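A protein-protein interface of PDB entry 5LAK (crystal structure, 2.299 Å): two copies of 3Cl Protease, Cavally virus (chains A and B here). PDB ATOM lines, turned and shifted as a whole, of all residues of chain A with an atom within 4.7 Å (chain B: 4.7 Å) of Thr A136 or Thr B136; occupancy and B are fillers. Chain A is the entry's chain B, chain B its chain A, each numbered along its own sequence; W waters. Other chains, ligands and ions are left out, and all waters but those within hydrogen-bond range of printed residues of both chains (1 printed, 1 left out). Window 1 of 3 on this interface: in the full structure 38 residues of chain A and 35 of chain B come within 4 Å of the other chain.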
ATOM      1  N   ASN A   5      -5.082  -8.779  24.594  1.00  0.00           N
ATOM      2  CA  ASN A   5      -4.692  -7.369  24.565  1.00  0.00           C
ATOM      3  C   ASN A   5      -5.221  -6.635  25.796  1.00  0.00           C
ATOM      4  O   ASN A   5      -6.433  -6.525  25.958  1.00  0.00           O
ATOM      5  CB  ASN A   5      -5.214  -6.697  23.294  1.00  0.00           C
ATOM      6  CG  ASN A   5      -4.734  -5.254  23.147  1.00  0.00           C
ATOM      7  OD1 ASN A   5      -4.215  -4.658  24.087  1.00  0.00           O
ATOM      8  ND2 ASN A   5      -4.913  -4.693  21.957  1.00  0.00           N
ATOM      9  N   HIS A  10      -6.248   5.031  28.344  1.00  0.00           N
ATOM     10  CA  HIS A  10      -5.446   6.185  28.738  1.00  0.00           C
ATOM     11  C   HIS A  10      -6.184   7.467  28.400  1.00  0.00           C
ATOM     12  O   HIS A  10      -6.694   7.622  27.290  1.00  0.00           O
ATOM     13  CB  HIS A  10      -4.082   6.171  28.040  1.00  0.00           C
ATOM     14  CG  HIS A  10      -3.179   5.063  28.490  1.00  0.00           C
ATOM     15  ND1 HIS A  10      -2.354   5.176  29.587  1.00  0.00           N
ATOM     16  CD2 HIS A  10      -2.961   3.826  27.982  1.00  0.00           C
ATOM     17  CE1 HIS A  10      -1.673   4.054  29.743  1.00  0.00           C
ATOM     18  NE2 HIS A  10      -2.022   3.218  28.781  1.00  0.00           N
ATOM     19  N   VAL A 116       1.402   2.802  31.457  1.00  0.00           N
ATOM     20  CA  VAL A 116       1.863   4.164  31.245  1.00  0.00           C
ATOM     21  C   VAL A 116       1.860   4.501  29.767  1.00  0.00           C
ATOM     22  O   VAL A 116       1.762   3.612  28.920  1.00  0.00           O
ATOM     23  CB  VAL A 116       3.287   4.379  31.791  1.00  0.00           C
ATOM     24  CG1 VAL A 116       3.330   4.121  33.289  1.00  0.00           C
ATOM     25  CG2 VAL A 116       4.281   3.477  31.062  1.00  0.00           C
ATOM     26  N   THR A 117       1.956   5.792  29.469  1.00  0.00           N
ATOM     27  CA  THR A 117       2.219   6.245  28.113  1.00  0.00           C
ATOM     28  C   THR A 117       3.549   6.985  28.054  1.00  0.00           C
ATOM     29  O   THR A 117       3.983   7.575  29.042  1.00  0.00           O
ATOM     30  CB  THR A 117       1.091   7.152  27.587  1.00  0.00           C
ATOM     31  OG1 THR A 117       0.758   8.138  28.574  1.00  0.00           O
ATOM     32  CG2 THR A 117      -0.141   6.320  27.271  1.00  0.00           C
ATOM     33  N   VAL A 134       2.649   9.254  20.842  1.00  0.00           N
ATOM     34  CA  VAL A 134       2.347   8.530  22.073  1.00  0.00           C
ATOM     35  C   VAL A 134       2.587   7.037  21.870  1.00  0.00           C
ATOM     36  O   VAL A 134       2.391   6.507  20.777  1.00  0.00           O
ATOM     37  CB  VAL A 134       0.888   8.778  22.540  1.00  0.00           C
ATOM     38  CG1 VAL A 134      -0.112   8.212  21.544  1.00  0.00           C
ATOM     39  CG2 VAL A 134       0.659   8.194  23.932  1.00  0.00           C
ATOM     40  N   HIS A 135       3.031   6.378  22.934  1.00  0.00           N
ATOM     41  CA  HIS A 135       3.287   4.940  22.941  1.00  0.00           C
ATOM     42  C   HIS A 135       2.754   4.354  24.241  1.00  0.00           C
ATOM     43  O   HIS A 135       2.816   5.014  25.274  1.00  0.00           O
ATOM     44  CB  HIS A 135       4.779   4.638  22.826  1.00  0.00           C
ATOM     45  CG  HIS A 135       5.504   5.515  21.857  1.00  0.00           C
ATOM     46  ND1 HIS A 135       5.751   6.848  22.101  1.00  0.00           N
ATOM     47  CD2 HIS A 135       6.073   5.238  20.660  1.00  0.00           C
ATOM     48  CE1 HIS A 135       6.419   7.362  21.083  1.00  0.00           C
ATOM     49  NE2 HIS A 135       6.629   6.405  20.197  1.00  0.00           N
ATOM     50  N   THR A 136       2.243   3.128  24.201  1.00  0.00           N
ATOM     51  CA  THR A 136       1.733   2.490  25.415  1.00  0.00           C
ATOM     52  C   THR A 136       2.698   1.440  25.946  1.00  0.00           C
ATOM     53  O   THR A 136       3.392   0.760  25.185  1.00  0.00           O
ATOM     54  CB  THR A 136       0.371   1.822  25.184  1.00  0.00           C
ATOM     55  OG1 THR A 136       0.459   0.919  24.079  1.00  0.00           O
ATOM     56  CG2 THR A 136      -0.695   2.873  24.915  1.00  0.00           C
ATOM     57  N   GLY A 137       2.723   1.310  27.266  1.00  0.00           N
ATOM     58  CA  GLY A 137       3.573   0.335  27.922  1.00  0.00           C
ATOM     59  C   GLY A 137       3.234   0.181  29.390  1.00  0.00           C
ATOM     60  O   GLY A 137       2.152   0.569  29.833  1.00  0.00           O
ATOM     61  N   ILE A 146       8.738   0.390  27.253  1.00  0.00           N
ATOM     62  CA  ILE A 146       8.546   1.006  25.946  1.00  0.00           C
ATOM     63  C   ILE A 146       9.889   1.184  25.244  1.00  0.00           C
ATOM     64  O   ILE A 146      10.796   1.815  25.785  1.00  0.00           O
ATOM     65  CB  ILE A 146       7.839   2.372  26.059  1.00  0.00           C
ATOM     66  CG1 ILE A 146       6.477   2.205  26.743  1.00  0.00           C
ATOM     67  CG2 ILE A 146       7.681   3.004  24.675  1.00  0.00           C
ATOM     68  CD1 ILE A 146       5.770   3.515  27.062  1.00  0.00           C
ATOM     69  N   ASN B   5       7.461  -5.520  23.760  1.00  0.00           N
ATOM     70  CA  ASN B   5       6.454  -4.466  23.604  1.00  0.00           C
ATOM     71  C   ASN B   5       6.611  -3.805  22.235  1.00  0.00           C
ATOM     72  O   ASN B   5       7.649  -3.195  21.973  1.00  0.00           O
ATOM     73  CB  ASN B   5       6.590  -3.421  24.714  1.00  0.00           C
ATOM     74  CG  ASN B   5       5.478  -2.378  24.691  1.00  0.00           C
ATOM     75  OD1 ASN B   5       4.720  -2.267  23.725  1.00  0.00           O
ATOM     76  ND2 ASN B   5       5.385  -1.599  25.766  1.00  0.00           N
ATOM     77  N   SER B   7       5.555  -1.165  21.125  1.00  0.00           N
ATOM     78  CA  SER B   7       5.893   0.225  21.403  1.00  0.00           C
ATOM     79  C   SER B   7       5.588   1.123  20.212  1.00  0.00           C
ATOM     80  O   SER B   7       6.368   2.011  19.881  1.00  0.00           O
ATOM     81  CB  SER B   7       7.369   0.339  21.787  1.00  0.00           C
ATOM     82  OG  SER B   7       7.674  -0.508  22.880  1.00  0.00           O
ATOM     83  N   HIS B  10       2.126   6.349  17.767  1.00  0.00           N
ATOM     84  CA  HIS B  10       0.871   6.882  17.248  1.00  0.00           C
ATOM     85  C   HIS B  10       0.901   8.400  17.352  1.00  0.00           C
ATOM     86  O   HIS B  10       1.229   8.953  18.401  1.00  0.00           O
ATOM     87  CB  HIS B  10      -0.328   6.319  18.011  1.00  0.00           C
ATOM     88  CG  HIS B  10      -0.526   4.844  17.829  1.00  0.00           C
ATOM     89  ND1 HIS B  10      -1.234   4.309  16.776  1.00  0.00           N
ATOM     90  CD2 HIS B  10      -0.122   3.793  18.582  1.00  0.00           C
ATOM     91  CE1 HIS B  10      -1.250   2.992  16.881  1.00  0.00           C
ATOM     92  NE2 HIS B  10      -0.582   2.654  17.969  1.00  0.00           N
ATOM     93  N   VAL B 116      -3.319   0.196  15.315  1.00  0.00           N
ATOM     94  CA  VAL B 116      -4.373   1.199  15.345  1.00  0.00           C
ATOM     95  C   VAL B 116      -4.570   1.731  16.750  1.00  0.00           C
ATOM     96  O   VAL B 116      -4.094   1.141  17.718  1.00  0.00           O
ATOM     97  CB  VAL B 116      -5.720   0.637  14.851  1.00  0.00           C
ATOM     98  CG1 VAL B 116      -5.607   0.168  13.419  1.00  0.00           C
ATOM     99  CG2 VAL B 116      -6.191  -0.501  15.756  1.00  0.00           C
ATOM    100  N   THR B 117      -5.280   2.846  16.848  1.00  0.00           N
ATOM    101  CA  THR B 117      -5.769   3.336  18.125  1.00  0.00           C
ATOM    102  C   THR B 117      -7.288   3.280  18.120  1.00  0.00           C
ATOM    103  O   THR B 117      -7.912   3.329  17.064  1.00  0.00           O
ATOM    104  CB  THR B 117      -5.330   4.783  18.418  1.00  0.00           C
ATOM    105  OG1 THR B 117      -5.565   5.602  17.267  1.00  0.00           O
ATOM    106  CG2 THR B 117      -3.860   4.843  18.790  1.00  0.00           C
ATOM    107  N   VAL B 134      -7.816   6.882  24.863  1.00  0.00           N
ATOM    108  CA  VAL B 134      -7.169   6.167  23.763  1.00  0.00           C
ATOM    109  C   VAL B 134      -6.715   4.773  24.188  1.00  0.00           C
ATOM    110  O   VAL B 134      -6.331   4.554  25.337  1.00  0.00           O
ATOM    111  CB  VAL B 134      -5.950   6.946  23.219  1.00  0.00           C
ATOM    112  CG1 VAL B 134      -4.850   7.054  24.274  1.00  0.00           C
ATOM    113  CG2 VAL B 134      -5.421   6.289  21.952  1.00  0.00           C
ATOM    114  N   HIS B 135      -6.771   3.838  23.245  1.00  0.00           N
ATOM    115  CA  HIS B 135      -6.332   2.467  23.470  1.00  0.00           C
ATOM    116  C   HIS B 135      -5.541   2.019  22.247  1.00  0.00           C
ATOM    117  O   HIS B 135      -5.898   2.372  21.124  1.00  0.00           O
ATOM    118  CB  HIS B 135      -7.521   1.525  23.687  1.00  0.00           C
ATOM    119  CG  HIS B 135      -8.629   2.119  24.502  1.00  0.00           C
ATOM    120  ND1 HIS B 135      -9.479   3.086  24.009  1.00  0.00           N
ATOM    121  CD2 HIS B 135      -9.027   1.880  25.774  1.00  0.00           C
ATOM    122  CE1 HIS B 135     -10.353   3.416  24.941  1.00  0.00           C
ATOM    123  NE2 HIS B 135     -10.100   2.701  26.023  1.00  0.00           N
ATOM    124  N   THR B 136      -4.493   1.224  22.456  1.00  0.00           N
ATOM    125  CA  THR B 136      -3.687   0.733  21.337  1.00  0.00           C
ATOM    126  C   THR B 136      -3.962  -0.731  21.025  1.00  0.00           C
ATOM    127  O   THR B 136      -4.225  -1.538  21.921  1.00  0.00           O
ATOM    128  CB  THR B 136      -2.186   0.905  21.606  1.00  0.00           C
ATOM    129  OG1 THR B 136      -1.853   0.320  22.870  1.00  0.00           O
ATOM    130  CG2 THR B 136      -1.822   2.380  21.615  1.00  0.00           C
ATOM    131  N   GLY B 137      -3.875  -1.065  19.739  1.00  0.00           N
ATOM    132  CA  GLY B 137      -4.099  -2.419  19.280  1.00  0.00           C
ATOM    133  C   GLY B 137      -3.687  -2.622  17.833  1.00  0.00           C
ATOM    134  O   GLY B 137      -2.900  -1.849  17.276  1.00  0.00           O
ATOM    135  N   ILE B 146      -8.769  -4.833  20.105  1.00  0.00           N
ATOM    136  CA  ILE B 146      -8.965  -3.978  21.271  1.00  0.00           C
ATOM    137  C   ILE B 146     -10.269  -4.357  21.984  1.00  0.00           C
ATOM    138  O   ILE B 146     -11.336  -4.376  21.374  1.00  0.00           O
ATOM    139  CB  ILE B 146      -8.963  -2.495  20.869  1.00  0.00           C
ATOM    140  CG1 ILE B 146      -7.625  -2.150  20.203  1.00  0.00           C
ATOM    141  CG2 ILE B 146      -9.204  -1.613  22.084  1.00  0.00           C
ATOM    142  CD1 ILE B 146      -7.545  -0.752  19.600  1.00  0.00           C
HETATM  143  O   HOH W   1       2.469  -0.995  23.238  1.00  0.00           O
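The side-chain amide nitrogen of Asn B5 sits at hydrogen-bond distance from the backbone carbonyl oxygen of Thr A136 (3.1 Å).
N of Val B134 lies within hydrogen-bond range of O of His A10 (2.8 Å).
The backbone carbonyl oxygen (O) of Thr B136 sits at hydrogen-bond distance from the side-chain amide nitrogen (ND2) of Asn A5, at 3.2 Å.
O of His B10 is in hydrogen-bond range of N of Val A134, 2.8 Å away.
OG1 of Thr B136 lies within hydrogen-bond range of OG1 of Thr A136 (2.7 Å).
OG of Ser B7 lies within hydrogen-bond range of O of Asn B5 (2.8 Å).
The backbone carbonyl oxygen (O) of Gly A137 lies within hydrogen-bond range of the backbone NH (N) of Val A116, 2.9 Å away.
N of Val B116 is in hydrogen-bond range of O of Gly B137 (2.9 Å).
Gly B137 touches Asn A5.
CD2 of His A135 touches O of Ser B7 (3.3 Å).
Gly A137 touches Asn B5 (CA to ND2, 3.4 Å).
Ile A146 touches Ser B7.
Printed residues of chain B within 4 Å of Asn A5: Thr B136 and Gly B137.
Printed residues of chain B within 4 Å of His A10: Val B134.
Thr A117 touches none of the printed residues of chain B.
Of the printed residues of chain B, His A135 touches Ser B7.
Of chain B, only Asn B5 (3.1 Å) and Thr B136 (2.7 Å) come within 4 Å of Thr A136.
Of the printed residues of chain B, Ile A146 touches Ser B7.
Printed residues of chain A within 4 Å of His B10: Val A134 (2.8 Å).
Of chain A, only Asn A5 (3.2 Å) and Thr A136 (2.7 Å) come within 4 Å of Thr B136.
The nearest residue of chain B that does not touch Thr A136 is Ser B7 (4.6 Å).
The nearest printed residue of chain A that does not touch Thr B136 is His A135 (5.6 Å).
The nearest printed residue of chain B that does not touch Ile A146 is Asn B5 (4.1 Å).
Printed residues of chain A that touch a printed residue of chain B: Asn A5, His A10, Val A134, His A135, Thr A136, Gly A137 and Ile A146.
Hydrophobic or aromatic side chains of chain A within 4 Å of the printed part of chain B: His A10, Val A134, His A135 and Ile A146.
Printed residues of chain B that touch a printed residue of chain A: Asn B5, Ser B7, His B10, Val B134, Thr B136 and Gly B137.
Along chain B the printed residues that touch a printed residue of chain A span positions 5 to 137.
Among the printed residues, 9 pairs touch across the chains.
Among the printed residues, no Asp or Glu carboxylate lies within 4 Å of a Lys or Arg side-chain nitrogen of the other chain.
Asn A5 touches Thr B136, and with the chains exchanged Thr A136 touches Asn B5.
Asn A5 touches Gly B137, and with the chains exchanged Gly A137 touches Asn B5.
His A10 touches Val B134, and with the chains exchanged Val A134 touches His B10.
Thr A136 touches its own counterpart, Thr B136.
Positions printed for both chains: 5, 10, 116, 117, 134, 135, 136, 137 and 146.
Of the 9 pairs that touch across the chains among the printed residues, 7 have their exchanged pair printed and touching as well.
Water W1 lies within hydrogen-bond range of OD1 of Asn B5 (2.6 Å) and O of Thr A136 (2.8 Å).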
